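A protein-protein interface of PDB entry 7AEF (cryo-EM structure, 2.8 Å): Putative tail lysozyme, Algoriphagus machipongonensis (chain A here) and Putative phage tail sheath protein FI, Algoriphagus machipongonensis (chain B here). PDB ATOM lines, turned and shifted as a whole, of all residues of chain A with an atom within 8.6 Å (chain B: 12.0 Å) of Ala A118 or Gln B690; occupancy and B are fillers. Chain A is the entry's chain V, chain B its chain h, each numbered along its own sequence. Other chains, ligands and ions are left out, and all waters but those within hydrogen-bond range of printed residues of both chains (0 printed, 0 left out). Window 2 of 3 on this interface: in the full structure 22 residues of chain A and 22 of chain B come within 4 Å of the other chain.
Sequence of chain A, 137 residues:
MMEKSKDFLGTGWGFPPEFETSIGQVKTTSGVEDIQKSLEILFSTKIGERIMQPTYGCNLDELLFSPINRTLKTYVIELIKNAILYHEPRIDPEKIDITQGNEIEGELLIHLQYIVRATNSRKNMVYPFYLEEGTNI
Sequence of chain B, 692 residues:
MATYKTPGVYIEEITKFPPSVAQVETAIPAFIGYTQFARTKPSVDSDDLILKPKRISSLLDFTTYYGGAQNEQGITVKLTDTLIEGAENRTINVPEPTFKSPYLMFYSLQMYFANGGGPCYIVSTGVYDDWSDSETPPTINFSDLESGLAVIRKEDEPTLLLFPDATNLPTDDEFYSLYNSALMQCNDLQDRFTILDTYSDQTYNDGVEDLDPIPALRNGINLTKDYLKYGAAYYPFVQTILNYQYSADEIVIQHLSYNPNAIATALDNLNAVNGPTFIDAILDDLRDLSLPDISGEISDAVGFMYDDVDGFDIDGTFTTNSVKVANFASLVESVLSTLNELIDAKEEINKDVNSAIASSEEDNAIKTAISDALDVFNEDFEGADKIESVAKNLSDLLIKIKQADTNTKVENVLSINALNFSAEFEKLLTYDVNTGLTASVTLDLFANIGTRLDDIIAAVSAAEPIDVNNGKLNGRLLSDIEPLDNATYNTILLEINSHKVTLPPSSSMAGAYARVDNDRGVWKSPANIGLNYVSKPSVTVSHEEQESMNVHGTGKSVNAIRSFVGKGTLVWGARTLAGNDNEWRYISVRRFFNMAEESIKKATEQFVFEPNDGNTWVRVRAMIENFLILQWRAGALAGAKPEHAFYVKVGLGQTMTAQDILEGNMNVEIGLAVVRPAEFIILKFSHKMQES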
ATOM      1  N   SER A   5      -4.157 -13.872  25.867  1.00  0.00           N
ATOM      2  CA  SER A   5      -3.910 -14.378  24.516  1.00  0.00           C
ATOM      3  C   SER A   5      -3.541 -13.258  23.521  1.00  0.00           C
ATOM      4  O   SER A   5      -2.638 -13.406  22.699  1.00  0.00           O
ATOM      5  CB  SER A   5      -5.123 -15.156  24.004  1.00  0.00           C
ATOM      6  OG  SER A   5      -6.279 -14.337  23.975  1.00  0.00           O
ATOM      7  N   LYS A   6      -4.267 -12.140  23.622  1.00  0.00           N
ATOM      8  CA  LYS A   6      -4.111 -10.966  22.769  1.00  0.00           C
ATOM      9  C   LYS A   6      -3.097  -9.997  23.380  1.00  0.00           C
ATOM     10  O   LYS A   6      -3.435  -8.881  23.753  1.00  0.00           O
ATOM     11  CB  LYS A   6      -5.456 -10.278  22.562  1.00  0.00           C
ATOM     12  CG  LYS A   6      -6.537 -11.163  21.980  1.00  0.00           C
ATOM     13  CD  LYS A   6      -7.853 -10.418  21.835  1.00  0.00           C
ATOM     14  CE  LYS A   6      -8.942 -11.317  21.283  1.00  0.00           C
ATOM     15  NZ  LYS A   6     -10.240 -10.605  21.141  1.00  0.00           N
ATOM     16  N   PHE A   8      -0.068  -9.428  21.679  1.00  0.00           N
ATOM     17  CA  PHE A   8       0.756  -8.860  20.611  1.00  0.00           C
ATOM     18  C   PHE A   8       0.161  -7.604  20.010  1.00  0.00           C
ATOM     19  O   PHE A   8       0.731  -7.052  19.066  1.00  0.00           O
ATOM     20  CB  PHE A   8       1.100  -9.878  19.490  1.00  0.00           C
ATOM     21  CG  PHE A   8      -0.054 -10.475  18.743  1.00  0.00           C
ATOM     22  CD1 PHE A   8      -0.686  -9.801  17.705  1.00  0.00           C
ATOM     23  CD2 PHE A   8      -0.420 -11.773  18.996  1.00  0.00           C
ATOM     24  CE1 PHE A   8      -1.697 -10.384  17.010  1.00  0.00           C
ATOM     25  CE2 PHE A   8      -1.430 -12.360  18.290  1.00  0.00           C
ATOM     26  CZ  PHE A   8      -2.068 -11.661  17.300  1.00  0.00           C
ATOM     27  N   LEU A   9      -0.965  -7.146  20.516  1.00  0.00           N
ATOM     28  CA  LEU A   9      -1.458  -5.864  20.071  1.00  0.00           C
ATOM     29  C   LEU A   9      -0.786  -4.786  20.890  1.00  0.00           C
ATOM     30  O   LEU A   9      -0.589  -3.664  20.417  1.00  0.00           O
ATOM     31  CB  LEU A   9      -2.989  -5.816  20.183  1.00  0.00           C
ATOM     32  CG  LEU A   9      -3.802  -6.862  19.390  1.00  0.00           C
ATOM     33  CD1 LEU A   9      -5.280  -6.671  19.662  1.00  0.00           C
ATOM     34  CD2 LEU A   9      -3.520  -6.780  17.893  1.00  0.00           C
ATOM     35  N   PRO A  89       0.192  -1.757  11.025  1.00  0.00           N
ATOM     36  CA  PRO A  89       0.296  -3.218  10.783  1.00  0.00           C
ATOM     37  C   PRO A  89      -0.779  -4.101  11.388  1.00  0.00           C
ATOM     38  O   PRO A  89      -0.859  -5.287  11.044  1.00  0.00           O
ATOM     39  CB  PRO A  89       1.639  -3.553  11.449  1.00  0.00           C
ATOM     40  CG  PRO A  89       2.369  -2.278  11.513  1.00  0.00           C
ATOM     41  CD  PRO A  89       1.363  -1.238  11.731  1.00  0.00           C
ATOM     42  N   ARG A  90      -1.545  -3.603  12.340  1.00  0.00           N
ATOM     43  CA  ARG A  90      -2.495  -4.453  13.029  1.00  0.00           C
ATOM     44  C   ARG A  90      -3.859  -4.569  12.353  1.00  0.00           C
ATOM     45  O   ARG A  90      -4.680  -5.357  12.829  1.00  0.00           O
ATOM     46  CB  ARG A  90      -2.641  -3.969  14.475  1.00  0.00           C
ATOM     47  CG  ARG A  90      -1.334  -4.154  15.284  1.00  0.00           C
ATOM     48  CD  ARG A  90      -1.336  -3.503  16.656  1.00  0.00           C
ATOM     49  NE  ARG A  90      -1.407  -2.047  16.550  1.00  0.00           N
ATOM     50  CZ  ARG A  90      -1.426  -1.177  17.564  1.00  0.00           C
ATOM     51  NH1 ARG A  90      -1.359  -1.563  18.827  1.00  0.00           N
ATOM     52  NH2 ARG A  90      -1.521   0.109  17.298  1.00  0.00           N
ATOM     53  N   ILE A  91      -4.170  -3.820  11.278  1.00  0.00           N
ATOM     54  CA  ILE A  91      -5.515  -3.906  10.702  1.00  0.00           C
ATOM     55  C   ILE A  91      -5.544  -4.111   9.190  1.00  0.00           C
ATOM     56  O   ILE A  91      -4.600  -3.794   8.469  1.00  0.00           O
ATOM     57  CB  ILE A  91      -6.384  -2.670  11.012  1.00  0.00           C
ATOM     58  CG1 ILE A  91      -5.834  -1.423  10.308  1.00  0.00           C
ATOM     59  CG2 ILE A  91      -6.493  -2.466  12.496  1.00  0.00           C
ATOM     60  CD1 ILE A  91      -6.752  -0.230  10.325  1.00  0.00           C
ATOM     61  N   ASP A  92      -6.707  -4.579   8.724  1.00  0.00           N
ATOM     62  CA  ASP A  92      -7.088  -4.694   7.309  1.00  0.00           C
ATOM     63  C   ASP A  92      -8.339  -3.869   7.041  1.00  0.00           C
ATOM     64  O   ASP A  92      -9.394  -4.162   7.627  1.00  0.00           O
ATOM     65  CB  ASP A  92      -7.382  -6.145   6.924  1.00  0.00           C
ATOM     66  CG  ASP A  92      -6.160  -6.998   6.747  1.00  0.00           C
ATOM     67  OD1 ASP A  92      -5.320  -6.697   5.898  1.00  0.00           O
ATOM     68  OD2 ASP A  92      -6.034  -7.995   7.472  1.00  0.00           O
ATOM     69  N   TYR A 114     -13.041  -1.223   9.336  1.00  0.00           N
ATOM     70  CA  TYR A 114     -11.869  -2.095   9.286  1.00  0.00           C
ATOM     71  C   TYR A 114     -11.996  -3.298  10.219  1.00  0.00           C
ATOM     72  O   TYR A 114     -12.799  -3.316  11.155  1.00  0.00           O
ATOM     73  CB  TYR A 114     -10.591  -1.324   9.629  1.00  0.00           C
ATOM     74  CG  TYR A 114     -10.553  -0.803  11.039  1.00  0.00           C
ATOM     75  CD1 TYR A 114      -9.961  -1.534  12.049  1.00  0.00           C
ATOM     76  CD2 TYR A 114     -11.094   0.428  11.354  1.00  0.00           C
ATOM     77  CE1 TYR A 114      -9.935  -1.082  13.319  1.00  0.00           C
ATOM     78  CE2 TYR A 114     -11.067   0.897  12.637  1.00  0.00           C
ATOM     79  CZ  TYR A 114     -10.479   0.137  13.616  1.00  0.00           C
ATOM     80  OH  TYR A 114     -10.433   0.577  14.911  1.00  0.00           O
ATOM     81  N   ILE A 115     -11.102  -4.267   9.993  1.00  0.00           N
ATOM     82  CA  ILE A 115     -11.034  -5.533  10.725  1.00  0.00           C
ATOM     83  C   ILE A 115      -9.686  -5.685  11.439  1.00  0.00           C
ATOM     84  O   ILE A 115      -8.625  -5.503  10.832  1.00  0.00           O
ATOM     85  CB  ILE A 115     -11.281  -6.705   9.763  1.00  0.00           C
ATOM     86  CG1 ILE A 115     -12.694  -6.578   9.187  1.00  0.00           C
ATOM     87  CG2 ILE A 115     -11.068  -8.046  10.455  1.00  0.00           C
ATOM     88  CD1 ILE A 115     -12.985  -7.451   8.010  1.00  0.00           C
ATOM     89  N   VAL A 116      -9.723  -6.062  12.715  1.00  0.00           N
ATOM     90  CA  VAL A 116      -8.508  -6.278  13.497  1.00  0.00           C
ATOM     91  C   VAL A 116      -7.955  -7.681  13.240  1.00  0.00           C
ATOM     92  O   VAL A 116      -8.689  -8.668  13.310  1.00  0.00           O
ATOM     93  CB  VAL A 116      -8.798  -6.034  14.988  1.00  0.00           C
ATOM     94  CG1 VAL A 116      -7.597  -6.353  15.841  1.00  0.00           C
ATOM     95  CG2 VAL A 116      -9.209  -4.586  15.187  1.00  0.00           C
ATOM     96  N   ARG A 117      -6.654  -7.772  12.941  1.00  0.00           N
ATOM     97  CA  ARG A 117      -5.992  -9.034  12.601  1.00  0.00           C
ATOM     98  C   ARG A 117      -5.827 -10.002  13.778  1.00  0.00           C
ATOM     99  O   ARG A 117      -5.400  -9.622  14.872  1.00  0.00           O
ATOM    100  CB  ARG A 117      -4.612  -8.736  12.021  1.00  0.00           C
ATOM    101  CG  ARG A 117      -4.667  -8.149  10.640  1.00  0.00           C
ATOM    102  CD  ARG A 117      -3.326  -7.735  10.147  1.00  0.00           C
ATOM    103  NE  ARG A 117      -3.417  -7.385   8.741  1.00  0.00           N
ATOM    104  CZ  ARG A 117      -2.497  -6.732   8.035  1.00  0.00           C
ATOM    105  NH1 ARG A 117      -1.371  -6.300   8.581  1.00  0.00           N
ATOM    106  NH2 ARG A 117      -2.719  -6.512   6.755  1.00  0.00           N
ATOM    107  N   ALA A 118      -6.094 -11.288  13.524  1.00  0.00           N
ATOM    108  CA  ALA A 118      -5.951 -12.355  14.516  1.00  0.00           C
ATOM    109  C   ALA A 118      -4.553 -12.964  14.581  1.00  0.00           C
ATOM    110  O   ALA A 118      -4.305 -13.821  15.433  1.00  0.00           O
ATOM    111  CB  ALA A 118      -6.941 -13.476  14.221  1.00  0.00           C
ATOM    112  N   THR A 119      -3.669 -12.626  13.649  1.00  0.00           N
ATOM    113  CA  THR A 119      -2.312 -13.159  13.559  1.00  0.00           C
ATOM    114  C   THR A 119      -1.342 -11.987  13.578  1.00  0.00           C
ATOM    115  O   THR A 119      -1.717 -10.908  13.171  1.00  0.00           O
ATOM    116  CB  THR A 119      -2.149 -13.972  12.259  1.00  0.00           C
ATOM    117  OG1 THR A 119      -3.101 -15.034  12.239  1.00  0.00           O
ATOM    118  CG2 THR A 119      -0.779 -14.573  12.105  1.00  0.00           C
ATOM    119  N   ASN A 120      -0.098 -12.177  14.033  1.00  0.00           N
ATOM    120  CA  ASN A 120       0.843 -11.085  14.221  1.00  0.00           C
ATOM    121  C   ASN A 120       1.660 -10.743  12.972  1.00  0.00           C
ATOM    122  O   ASN A 120       2.364 -11.594  12.420  1.00  0.00           O
ATOM    123  CB  ASN A 120       1.775 -11.389  15.372  1.00  0.00           C
ATOM    124  CG  ASN A 120       2.517 -10.197  15.744  1.00  0.00           C
ATOM    125  OD1 ASN A 120       2.011  -9.091  15.576  1.00  0.00           O
ATOM    126  ND2 ASN A 120       3.724 -10.366  16.196  1.00  0.00           N
ATOM    127  N   SER A 121       1.577  -9.476  12.564  1.00  0.00           N
ATOM    128  CA  SER A 121       2.289  -8.924  11.415  1.00  0.00           C
ATOM    129  C   SER A 121       3.790  -8.788  11.643  1.00  0.00           C
ATOM    130  O   SER A 121       4.250  -8.483  12.740  1.00  0.00           O
ATOM    131  CB  SER A 121       1.758  -7.540  11.086  1.00  0.00           C
ATOM    132  OG  SER A 121       2.591  -6.947  10.121  1.00  0.00           O
ATOM    133  N   SER B 686     -14.765   2.608  12.518  1.00  0.00           N
ATOM    134  CA  SER B 686     -15.449   1.560  13.256  1.00  0.00           C
ATOM    135  C   SER B 686     -14.761   0.239  12.922  1.00  0.00           C
ATOM    136  O   SER B 686     -14.155   0.093  11.862  1.00  0.00           O
ATOM    137  CB  SER B 686     -16.914   1.457  12.878  1.00  0.00           C
ATOM    138  OG  SER B 686     -17.075   1.144  11.529  1.00  0.00           O
ATOM    139  N   HIS B 687     -14.915  -0.737  13.800  1.00  0.00           N
ATOM    140  CA  HIS B 687     -14.232  -2.004  13.654  1.00  0.00           C
ATOM    141  C   HIS B 687     -15.089  -3.223  13.935  1.00  0.00           C
ATOM    142  O   HIS B 687     -16.134  -3.143  14.552  1.00  0.00           O
ATOM    143  CB  HIS B 687     -13.094  -2.041  14.642  1.00  0.00           C
ATOM    144  CG  HIS B 687     -13.499  -2.559  15.981  1.00  0.00           C
ATOM    145  ND1 HIS B 687     -14.074  -1.761  16.944  1.00  0.00           N
ATOM    146  CD2 HIS B 687     -13.412  -3.798  16.522  1.00  0.00           C
ATOM    147  CE1 HIS B 687     -14.340  -2.487  18.012  1.00  0.00           C
ATOM    148  NE2 HIS B 687     -13.946  -3.726  17.782  1.00  0.00           N
ATOM    149  N   LYS B 688     -14.604  -4.363  13.451  1.00  0.00           N
ATOM    150  CA  LYS B 688     -15.136  -5.683  13.760  1.00  0.00           C
ATOM    151  C   LYS B 688     -13.980  -6.623  14.041  1.00  0.00           C
ATOM    152  O   LYS B 688     -12.869  -6.397  13.567  1.00  0.00           O
ATOM    153  CB  LYS B 688     -15.958  -6.232  12.608  1.00  0.00           C
ATOM    154  CG  LYS B 688     -17.185  -5.439  12.303  1.00  0.00           C
ATOM    155  CD  LYS B 688     -17.978  -6.072  11.187  1.00  0.00           C
ATOM    156  CE  LYS B 688     -19.221  -5.257  10.864  1.00  0.00           C
ATOM    157  NZ  LYS B 688     -20.009  -5.861   9.751  1.00  0.00           N
ATOM    158  N   MET B 689     -14.235  -7.677  14.804  1.00  0.00           N
ATOM    159  CA  MET B 689     -13.217  -8.689  15.062  1.00  0.00           C
ATOM    160  C   MET B 689     -13.242  -9.728  13.963  1.00  0.00           C
ATOM    161  O   MET B 689     -14.309 -10.087  13.470  1.00  0.00           O
ATOM    162  CB  MET B 689     -13.447  -9.366  16.409  1.00  0.00           C
ATOM    163  CG  MET B 689     -13.392  -8.434  17.603  1.00  0.00           C
ATOM    164  SD  MET B 689     -11.811  -7.594  17.804  1.00  0.00           S
ATOM    165  CE  MET B 689     -10.702  -8.912  18.276  1.00  0.00           C
ATOM    166  N   GLN B 690     -12.080 -10.231  13.597  1.00  0.00           N
ATOM    167  CA  GLN B 690     -12.026 -11.258  12.575  1.00  0.00           C
ATOM    168  C   GLN B 690     -12.845 -12.475  12.983  1.00  0.00           C
ATOM    169  O   GLN B 690     -12.343 -13.383  13.631  1.00  0.00           O
ATOM    170  CB  GLN B 690     -10.580 -11.652  12.294  1.00  0.00           C
ATOM    171  CG  GLN B 690     -10.406 -12.625  11.157  1.00  0.00           C
ATOM    172  CD  GLN B 690      -8.957 -12.875  10.839  1.00  0.00           C
ATOM    173  OE1 GLN B 690      -8.064 -12.302  11.460  1.00  0.00           O
ATOM    174  NE2 GLN B 690      -8.710 -13.730   9.861  1.00  0.00           N
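N of Arg A117 sits at hydrogen-bond distance from O of Arg A90, at 3.1 Å.
The backbone carbonyl oxygen (O) of Pro A89 sits at hydrogen-bond distance from the guanidinium group (NH1) of Arg A117 (2.7 Å).
O of Asp A92 lies within hydrogen-bond range of N of Ile A115.
The guanidinium group of Arg A117 is in salt-bridge range of the side-chain carboxylate of Asp A92, at 2.7 Å.
Among the printed residues, merely in contact across the chains: Tyr A114 with His B687 (3.2 Å), Lys A6 with Met B689 (3.4 Å), Ile A115 with Lys B688 (3.5 Å), Val A116 with Gln B690 (3.7 Å), Arg A117 with Gln B690 (3.96 Å) and Ile A115 with Gln B690 (3.96 Å).
Of the 16 printed residues of chain A, 6 touch a printed residue of chain B.
Hydrophobic or aromatic side chains of chain A that line the printed part of chain B: Tyr A114, Ile A115 and Ala A118.
Printed residues of chain B that touch a printed residue of chain A: Ser B686, His B687, Lys B688, Met B689 and Gln B690.
Hydrophobic or aromatic side chains of chain B within 4 Å of the printed part of chain A: His B687 and Met B689.
Among the printed residues, no Asp or Glu carboxylate lies within 4 Å of a Lys or Arg side-chain nitrogen of the other chain.
N of Val A116 is in hydrogen-bond range of O of Lys B688, at 3.3 Å.
The backbone NH (N) of Ala A118 is in hydrogen-bond range of the side-chain amide oxygen (OE1) of Gln B690.
O of Tyr A114 is in hydrogen-bond range of N of Lys B688 (3.1 Å).
O of Ser B686 is in hydrogen-bond range of N of Tyr A114 (3.1 Å).
Ile A115 touches two residues of chain B.
Of chain B, only Lys B688 and Gln B690 come within 4 Å of Val A116.
Of chain B, only Gln B690 comes within 4 Å of Ala A118.
Thr A119 touches none of the printed residues of chain B.
Asn A120 touches none of the printed residues of chain B.
Printed residues of chain A within 4 Å of Ser B686: Tyr A114.
Of the printed residues of chain A, His B687 touches Tyr A114 (3.2 Å).
Of chain A, only Ile A115 (3.96 Å), Val A116 (3.7 Å), Arg A117 (3.96 Å) and Ala A118 (3.0 Å) come within 4 Å of Gln B690.
The nearest residue of chain A that does not touch Gln B690 is Thr A119 (4.9 Å).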
